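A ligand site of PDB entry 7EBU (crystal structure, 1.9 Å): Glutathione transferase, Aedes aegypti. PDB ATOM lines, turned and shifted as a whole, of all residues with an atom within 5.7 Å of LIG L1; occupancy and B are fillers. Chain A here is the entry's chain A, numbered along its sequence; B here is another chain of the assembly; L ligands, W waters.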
ATOM      1  N   SER A  19     -17.452 -14.727 -32.078  1.00  0.00           N
ATOM      2  CA  SER A  19     -18.838 -14.860 -31.665  1.00  0.00           C
ATOM      3  C   SER A  19     -19.469 -13.485 -31.467  1.00  0.00           C
ATOM      4  O   SER A  19     -18.915 -12.662 -30.724  1.00  0.00           O
ATOM      5  CB  SER A  19     -18.911 -15.631 -30.360  1.00  0.00           C
ATOM      6  OG  SER A  19     -20.110 -15.349 -29.662  1.00  0.00           O
ATOM      7  N   PRO A  20     -20.607 -13.198 -32.099  1.00  0.00           N
ATOM      8  CA  PRO A  20     -21.331 -11.914 -31.846  1.00  0.00           C
ATOM      9  C   PRO A  20     -21.673 -11.717 -30.378  1.00  0.00           C
ATOM     10  O   PRO A  20     -21.451 -10.614 -29.848  1.00  0.00           O
ATOM     11  CB  PRO A  20     -22.585 -12.027 -32.712  1.00  0.00           C
ATOM     12  CG  PRO A  20     -22.234 -12.993 -33.786  1.00  0.00           C
ATOM     13  CD  PRO A  20     -21.203 -13.962 -33.206  1.00  0.00           C
ATOM     14  N   PRO A  21     -22.249 -12.703 -29.672  1.00  0.00           N
ATOM     15  CA  PRO A  21     -22.478 -12.498 -28.223  1.00  0.00           C
ATOM     16  C   PRO A  21     -21.245 -12.034 -27.455  1.00  0.00           C
ATOM     17  O   PRO A  21     -21.304 -11.135 -26.590  1.00  0.00           O
ATOM     18  CB  PRO A  21     -22.933 -13.880 -27.738  1.00  0.00           C
ATOM     19  CG  PRO A  21     -23.629 -14.452 -28.918  1.00  0.00           C
ATOM     20  CD  PRO A  21     -22.828 -13.992 -30.124  1.00  0.00           C
ATOM     21  N   LEU A  45     -13.308 -21.473 -30.380  1.00  0.00           N
ATOM     22  CA  LEU A  45     -14.373 -22.357 -30.853  1.00  0.00           C
ATOM     23  C   LEU A  45     -13.867 -23.297 -31.946  1.00  0.00           C
ATOM     24  O   LEU A  45     -14.140 -24.500 -31.917  1.00  0.00           O
ATOM     25  CB  LEU A  45     -15.547 -21.518 -31.350  1.00  0.00           C
ATOM     26  CG  LEU A  45     -16.265 -20.695 -30.275  1.00  0.00           C
ATOM     27  CD1 LEU A  45     -17.304 -19.752 -30.906  1.00  0.00           C
ATOM     28  CD2 LEU A  45     -16.909 -21.593 -29.244  1.00  0.00           C
ATOM     29  N   HIS A  50     -14.100 -25.156 -26.290  1.00  0.00           N
ATOM     30  CA  HIS A  50     -15.348 -25.068 -25.544  1.00  0.00           C
ATOM     31  C   HIS A  50     -15.931 -26.414 -25.187  1.00  0.00           C
ATOM     32  O   HIS A  50     -16.937 -26.462 -24.464  1.00  0.00           O
ATOM     33  CB  HIS A  50     -16.394 -24.251 -26.345  1.00  0.00           C
ATOM     34  CG  HIS A  50     -16.737 -24.847 -27.674  1.00  0.00           C
ATOM     35  ND1 HIS A  50     -15.828 -24.990 -28.696  1.00  0.00           N
ATOM     36  CD2 HIS A  50     -17.920 -25.310 -28.162  1.00  0.00           C
ATOM     37  CE1 HIS A  50     -16.413 -25.548 -29.739  1.00  0.00           C
ATOM     38  NE2 HIS A  50     -17.693 -25.737 -29.448  1.00  0.00           N
ATOM     39  N   LEU A  51     -15.345 -27.510 -25.676  1.00  0.00           N
ATOM     40  CA  LEU A  51     -15.831 -28.848 -25.365  1.00  0.00           C
ATOM     41  C   LEU A  51     -14.941 -29.565 -24.353  1.00  0.00           C
ATOM     42  O   LEU A  51     -15.197 -30.719 -24.049  1.00  0.00           O
ATOM     43  CB  LEU A  51     -15.955 -29.689 -26.639  1.00  0.00           C
ATOM     44  CG  LEU A  51     -16.841 -29.075 -27.743  1.00  0.00           C
ATOM     45  CD1 LEU A  51     -16.811 -29.892 -29.037  1.00  0.00           C
ATOM     46  CD2 LEU A  51     -18.257 -28.889 -27.250  1.00  0.00           C
ATOM     47  N   LEU A  61     -23.886 -25.506 -21.513  1.00  0.00           N
ATOM     48  CA  LEU A  61     -24.210 -25.083 -22.869  1.00  0.00           C
ATOM     49  C   LEU A  61     -22.980 -25.061 -23.778  1.00  0.00           C
ATOM     50  O   LEU A  61     -23.118 -24.908 -25.002  1.00  0.00           O
ATOM     51  CB  LEU A  61     -24.869 -23.692 -22.832  1.00  0.00           C
ATOM     52  CG  LEU A  61     -26.247 -23.536 -22.149  1.00  0.00           C
ATOM     53  CD1 LEU A  61     -26.630 -22.058 -21.899  1.00  0.00           C
ATOM     54  CD2 LEU A  61     -27.311 -24.252 -22.967  1.00  0.00           C
ATOM     55  N   HIS A  62     -21.787 -25.215 -23.193  1.00  0.00           N
ATOM     56  CA  HIS A  62     -20.517 -25.239 -23.919  1.00  0.00           C
ATOM     57  C   HIS A  62     -20.467 -24.152 -24.989  1.00  0.00           C
ATOM     58  O   HIS A  62     -20.252 -24.399 -26.180  1.00  0.00           O
ATOM     59  CB  HIS A  62     -20.236 -26.630 -24.511  1.00  0.00           C
ATOM     60  CG  HIS A  62     -21.348 -27.198 -25.330  1.00  0.00           C
ATOM     61  ND1 HIS A  62     -21.590 -26.808 -26.635  1.00  0.00           N
ATOM     62  CD2 HIS A  62     -22.282 -28.135 -25.050  1.00  0.00           C
ATOM     63  CE1 HIS A  62     -22.630 -27.461 -27.110  1.00  0.00           C
ATOM     64  NE2 HIS A  62     -23.074 -28.282 -26.162  1.00  0.00           N
ATOM     65  N   ALA A  63     -20.682 -22.922 -24.550  1.00  0.00           N
ATOM     66  CA  ALA A  63     -20.781 -21.788 -25.450  1.00  0.00           C
ATOM     67  C   ALA A  63     -20.086 -20.596 -24.803  1.00  0.00           C
ATOM     68  O   ALA A  63     -19.945 -20.527 -23.580  1.00  0.00           O
ATOM     69  CB  ALA A  63     -22.242 -21.442 -25.775  1.00  0.00           C
ATOM     70  N   VAL A  64     -19.657 -19.657 -25.634  1.00  0.00           N
ATOM     71  CA  VAL A  64     -19.057 -18.414 -25.149  1.00  0.00           C
ATOM     72  C   VAL A  64     -19.999 -17.271 -25.524  1.00  0.00           C
ATOM     73  O   VAL A  64     -20.703 -17.357 -26.549  1.00  0.00           O
ATOM     74  CB  VAL A  64     -17.654 -18.235 -25.726  1.00  0.00           C
ATOM     75  CG1 VAL A  64     -16.717 -19.342 -25.208  1.00  0.00           C
ATOM     76  CG2 VAL A  64     -17.683 -18.207 -27.243  1.00  0.00           C
ATOM     77  N   PRO A  65     -20.050 -16.207 -24.743  1.00  0.00           N
ATOM     78  CA  PRO A  65     -19.188 -15.962 -23.572  1.00  0.00           C
ATOM     79  C   PRO A  65     -19.653 -16.538 -22.254  1.00  0.00           C
ATOM     80  O   PRO A  65     -20.831 -16.847 -22.062  1.00  0.00           O
ATOM     81  CB  PRO A  65     -19.174 -14.439 -23.476  1.00  0.00           C
ATOM     82  CG  PRO A  65     -20.591 -14.063 -23.965  1.00  0.00           C
ATOM     83  CD  PRO A  65     -20.924 -15.037 -25.048  1.00  0.00           C
ATOM     84  N   THR A  75     -23.794 -17.323 -18.035  1.00  0.00           N
ATOM     85  CA  THR A  75     -23.618 -18.125 -19.232  1.00  0.00           C
ATOM     86  C   THR A  75     -24.485 -17.594 -20.355  1.00  0.00           C
ATOM     87  O   THR A  75     -24.984 -18.364 -21.181  1.00  0.00           O
ATOM     88  CB  THR A  75     -23.917 -19.598 -18.947  1.00  0.00           C
ATOM     89  OG1 THR A  75     -25.253 -19.741 -18.451  1.00  0.00           O
ATOM     90  CG2 THR A  75     -22.939 -20.129 -17.855  1.00  0.00           C
ATOM     91  N   ASP A  76     -24.654 -16.274 -20.394  1.00  0.00           N
ATOM     92  CA  ASP A  76     -25.320 -15.608 -21.502  1.00  0.00           C
ATOM     93  C   ASP A  76     -24.793 -14.191 -21.583  1.00  0.00           C
ATOM     94  O   ASP A  76     -24.791 -13.471 -20.587  1.00  0.00           O
ATOM     95  CB  ASP A  76     -26.840 -15.644 -21.327  1.00  0.00           C
ATOM     96  CG  ASP A  76     -27.571 -15.242 -22.600  1.00  0.00           C
ATOM     97  OD1 ASP A  76     -27.506 -14.049 -22.937  1.00  0.00           O
ATOM     98  OD2 ASP A  76     -28.182 -16.124 -23.246  1.00  0.00           O
ATOM     99  N   SER A  77     -24.325 -13.815 -22.783  1.00  0.00           N
ATOM    100  CA  SER A  77     -23.762 -12.490 -23.013  1.00  0.00           C
ATOM    101  C   SER A  77     -24.652 -11.381 -22.452  1.00  0.00           C
ATOM    102  O   SER A  77     -24.143 -10.374 -21.935  1.00  0.00           O
ATOM    103  CB  SER A  77     -23.536 -12.282 -24.502  1.00  0.00           C
ATOM    104  OG  SER A  77     -24.750 -12.187 -25.228  1.00  0.00           O
ATOM    105  N   HIS A  78     -25.977 -11.553 -22.563  1.00  0.00           N
ATOM    106  CA  HIS A  78     -26.909 -10.498 -22.162  1.00  0.00           C
ATOM    107  C   HIS A  78     -26.959 -10.338 -20.646  1.00  0.00           C
ATOM    108  O   HIS A  78     -26.968  -9.206 -20.138  1.00  0.00           O
ATOM    109  CB  HIS A  78     -28.294 -10.804 -22.765  1.00  0.00           C
ATOM    110  CG  HIS A  78     -28.249 -10.952 -24.262  1.00  0.00           C
ATOM    111  ND1 HIS A  78     -27.900 -12.136 -24.880  1.00  0.00           N
ATOM    112  CD2 HIS A  78     -28.359 -10.037 -25.261  1.00  0.00           C
ATOM    113  CE1 HIS A  78     -27.885 -11.966 -26.189  1.00  0.00           C
ATOM    114  NE2 HIS A  78     -28.161 -10.697 -26.454  1.00  0.00           N
ATOM    115  N   ASN A 113     -31.263 -11.320 -28.096  1.00  0.00           N
ATOM    116  CA  ASN A 113     -31.038 -12.721 -27.713  1.00  0.00           C
ATOM    117  C   ASN A 113     -32.030 -13.643 -28.407  1.00  0.00           C
ATOM    118  O   ASN A 113     -31.657 -14.684 -28.967  1.00  0.00           O
ATOM    119  CB  ASN A 113     -31.150 -12.863 -26.199  1.00  0.00           C
ATOM    120  CG  ASN A 113     -30.345 -14.036 -25.641  1.00  0.00           C
ATOM    121  OD1 ASN A 113     -29.519 -14.645 -26.337  1.00  0.00           O
ATOM    122  ND2 ASN A 113     -30.586 -14.350 -24.363  1.00  0.00           N
ATOM    123  N   PHE A 117     -30.266 -12.439 -32.763  1.00  0.00           N
ATOM    124  CA  PHE A 117     -29.178 -13.408 -32.738  1.00  0.00           C
ATOM    125  C   PHE A 117     -29.658 -14.817 -33.090  1.00  0.00           C
ATOM    126  O   PHE A 117     -28.913 -15.578 -33.714  1.00  0.00           O
ATOM    127  CB  PHE A 117     -28.471 -13.447 -31.383  1.00  0.00           C
ATOM    128  CG  PHE A 117     -27.467 -14.572 -31.272  1.00  0.00           C
ATOM    129  CD1 PHE A 117     -26.295 -14.525 -32.024  1.00  0.00           C
ATOM    130  CD2 PHE A 117     -27.720 -15.689 -30.486  1.00  0.00           C
ATOM    131  CE1 PHE A 117     -25.369 -15.558 -31.957  1.00  0.00           C
ATOM    132  CE2 PHE A 117     -26.803 -16.711 -30.417  1.00  0.00           C
ATOM    133  CZ  PHE A 117     -25.632 -16.640 -31.151  1.00  0.00           C
ATOM    134  N   GLN A 118     -30.891 -15.189 -32.718  1.00  0.00           N
ATOM    135  CA  GLN A 118     -31.377 -16.525 -33.090  1.00  0.00           C
ATOM    136  C   GLN A 118     -31.395 -16.708 -34.598  1.00  0.00           C
ATOM    137  O   GLN A 118     -30.870 -17.695 -35.137  1.00  0.00           O
ATOM    138  CB  GLN A 118     -32.785 -16.763 -32.521  1.00  0.00           C
ATOM    139  CG  GLN A 118     -32.839 -16.825 -31.004  1.00  0.00           C
ATOM    140  CD  GLN A 118     -31.856 -17.818 -30.373  1.00  0.00           C
ATOM    141  OE1 GLN A 118     -31.263 -17.559 -29.315  1.00  0.00           O
ATOM    142  NE2 GLN A 118     -31.694 -18.971 -31.018  1.00  0.00           N
ATOM    143  N   SER A 121     -27.845 -16.581 -36.111  1.00  0.00           N
ATOM    144  CA  SER A 121     -27.095 -17.777 -35.788  1.00  0.00           C
ATOM    145  C   SER A 121     -27.503 -18.927 -36.690  1.00  0.00           C
ATOM    146  O   SER A 121     -26.653 -19.682 -37.152  1.00  0.00           O
ATOM    147  CB  SER A 121     -27.332 -18.142 -34.329  1.00  0.00           C
ATOM    148  OG  SER A 121     -26.499 -19.212 -33.934  1.00  0.00           O
ATOM    149  N   ALA B 114     -33.581 -17.965 -24.720  1.00  0.00           N
ATOM    150  CA  ALA B 114     -32.704 -18.240 -25.851  1.00  0.00           C
ATOM    151  C   ALA B 114     -32.479 -19.723 -26.106  1.00  0.00           C
ATOM    152  O   ALA B 114     -31.978 -20.071 -27.189  1.00  0.00           O
ATOM    153  CB  ALA B 114     -31.348 -17.572 -25.651  1.00  0.00           C
HETATM  154  N1  LIG L   1     -27.581 -16.663 -25.900  1.00  0.00           N
HETATM  155  C1  LIG L   1     -26.105 -16.888 -25.796  1.00  0.00           C
HETATM  156  C2  LIG L   1     -25.366 -15.598 -25.418  1.00  0.00           C
HETATM  157  O1  LIG L   1     -25.857 -14.512 -25.812  1.00  0.00           O
HETATM  158  O2  LIG L   1     -24.307 -15.705 -24.744  1.00  0.00           O
HETATM  159  C3  LIG L   1     -25.593 -17.487 -27.108  1.00  0.00           C
HETATM  160  C4  LIG L   1     -24.105 -17.822 -27.073  1.00  0.00           C
HETATM  161  C5  LIG L   1     -23.700 -18.663 -28.259  1.00  0.00           C
HETATM  162  O3  LIG L   1     -24.520 -19.209 -28.986  1.00  0.00           O
HETATM  163  N2  LIG L   1     -22.387 -18.771 -28.476  1.00  0.00           N
HETATM  164  C6  LIG L   1     -21.833 -19.526 -29.576  1.00  0.00           C
HETATM  165  C7  LIG L   1     -21.023 -20.747 -29.142  1.00  0.00           C
HETATM  166  O4  LIG L   1     -20.181 -20.610 -28.254  1.00  0.00           O
HETATM  167  C8  LIG L   1     -20.972 -18.669 -30.485  1.00  0.00           C
HETATM  168  S1  LIG L   1     -21.900 -17.384 -31.357  1.00  0.00           S
HETATM  169  N3  LIG L   1     -21.253 -21.881 -29.801  1.00  0.00           N
HETATM  170  C9  LIG L   1     -20.540 -23.114 -29.507  1.00  0.00           C
HETATM  171  C10 LIG L   1     -21.501 -24.291 -29.344  1.00  0.00           C
HETATM  172  O5  LIG L   1     -22.706 -24.058 -29.542  1.00  0.00           O
HETATM  173  O6  LIG L   1     -21.009 -25.405 -29.045  1.00  0.00           O
HETATM  174  O1  LG2 L   2     -22.490 -15.481 -35.764  1.00  0.00           O
HETATM  175  C1  LG2 L   2     -22.056 -16.720 -35.478  1.00  0.00           C
HETATM  176  C2  LG2 L   2     -22.994 -17.754 -35.311  1.00  0.00           C
HETATM  177  C3  LG2 L   2     -22.567 -19.050 -35.008  1.00  0.00           C
HETATM  178  C4  LG2 L   2     -21.204 -19.303 -34.877  1.00  0.00           C
HETATM  179  C5  LG2 L   2     -20.214 -18.195 -35.044  1.00  0.00           C
HETATM  180  C6  LG2 L   2     -20.680 -16.925 -35.342  1.00  0.00           C
HETATM  181  O2  LG2 L   2     -18.878 -18.455 -34.906  1.00  0.00           O
HETATM  182  C7  LG2 L   2     -18.396 -19.671 -34.616  1.00  0.00           C
HETATM  183  C8  LG2 L   2     -19.203 -20.786 -34.421  1.00  0.00           C
HETATM  184  C9  LG2 L   2     -20.669 -20.634 -34.542  1.00  0.00           C
HETATM  185  O3  LG2 L   2     -21.439 -21.594 -34.389  1.00  0.00           O
HETATM  186  C10 LG2 L   2     -18.559 -22.101 -34.110  1.00  0.00           C
HETATM  187  C11 LG2 L   2     -17.451 -22.503 -34.848  1.00  0.00           C
HETATM  188  C12 LG2 L   2     -16.841 -23.726 -34.588  1.00  0.00           C
HETATM  189  C13 LG2 L   2     -17.328 -24.548 -33.580  1.00  0.00           C
HETATM  190  O4  LG2 L   2     -16.731 -25.739 -33.341  1.00  0.00           O
HETATM  191  C14 LG2 L   2     -18.453 -24.162 -32.836  1.00  0.00           C
HETATM  192  C15 LG2 L   2     -19.059 -22.926 -33.099  1.00  0.00           C
HETATM  193  O   HOH W   1     -22.716 -17.800 -23.793  1.00  0.00           O
HETATM  194  O   HOH W   2     -24.864 -22.160 -29.240  1.00  0.00           O
HETATM  195  O   HOH W   3     -27.944 -19.325 -25.038  1.00  0.00           O
HETATM  196  O   HOH W   4     -26.718 -20.099 -29.668  1.00  0.00           O
HETATM  197  O   HOH W   5     -22.777 -21.910 -32.144  1.00  0.00           O
HETATM  198  O   HOH W   6     -28.744 -18.759 -27.524  1.00  0.00           O
HETATM  199  O   HOH W   7     -24.772 -25.648 -29.249  1.00  0.00           O
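N of Ser 77 is in hydrogen-bond range of O2 of LIG L1, 2.7 Å away. OG of Ser 77 sits at hydrogen-bond distance from O1 of LIG L1. N1 of LIG L1 lies within salt-bridge range of OD2 of Asp 76, 2.8 Å away. N1 of LIG L1 sits at hydrogen-bond distance from OD1 of Asn 113. The backbone NH of Val 64 lies within hydrogen-bond range of an oxygen (O4) of LIG L1 (2.8 Å). The backbone carbonyl oxygen of Val 64 sits at hydrogen-bond distance from a nitrogen (N2) of LIG L1 (2.9 Å). ND1 of His 62 sits at hydrogen-bond distance from O6 of LIG L1 (2.8 Å). A sulfur (S1) of LIG L1 sits close to the side-chain hydroxyl (OG) of Ser 19, 3.2 Å away. A ring nitrogen (NE2) of His 50 sits close to an oxygen (O6) of LIG L1 (3.4 Å). An oxygen (O1) of LIG L1 is in hydrogen-bond range of a ring nitrogen (ND1) of His 78 (3.3 Å). O of Leu 45 sits at hydrogen-bond distance from O4 of LG2 L2 (3.2 Å).
Water W5 bridges O3 of LG2 L2 (2.6 Å) and N3 of LIG L1 (2.8 Å). Water W1 lies within hydrogen-bond range of the backbone carbonyl oxygen (O) of Pro 65, an oxygen (O2) of LIG L1 and the backbone carbonyl oxygen (O) of Val 64. Water W6 bridges N1 of LIG L1 and OE1 of Gln 118.
ND1 of His 78 sits at hydrogen-bond distance from OG of Ser 77 (3.2 Å). The side-chain carboxylate (OD2) of Asp 76 lies within hydrogen-bond range of the side-chain amide nitrogen (ND2) of Asn 113 (3.2 Å). The side-chain carboxylate of Asp 76 is in hydrogen-bond range of a ring nitrogen (ND1) of His 78. A ring nitrogen (ND1) of His 78 lies close to the side-chain amide oxygen (OD1) of Asn 113. O of Asn 113 sits close to OE1 of Gln 118 (2.9 Å). The side-chain amide oxygen (OE1) of Gln 118 sits close to the backbone carbonyl oxygen (O) of Ala 114 of chain B (3.4 Å).
CD of Pro 20 touches S1 of LIG L1 (3.95 Å). Pro 21 touches LIG L1 (CB to O1, 3.6 Å). CD2 of Leu 45 touches O4 of LIG L1, at 3.6 Å. CA of Ala 63 touches O4 of LIG L1, at 3.1 Å. Pro 65 touches LIG L1 (CD to O2, 3.5 Å). Phe 117 touches LIG L1. CB of Ala 114 of chain B touches N1 of LIG L1 (3.9 Å). Within 4 Å of LIG L1: Ser 19, Pro 20, Pro 21, Leu 45, His 50, His 62, Ala 63, Val 64, Pro 65, Asp 76, Ser 77, His 78, Asn 113, Phe 117 and Ala 114 of chain B.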
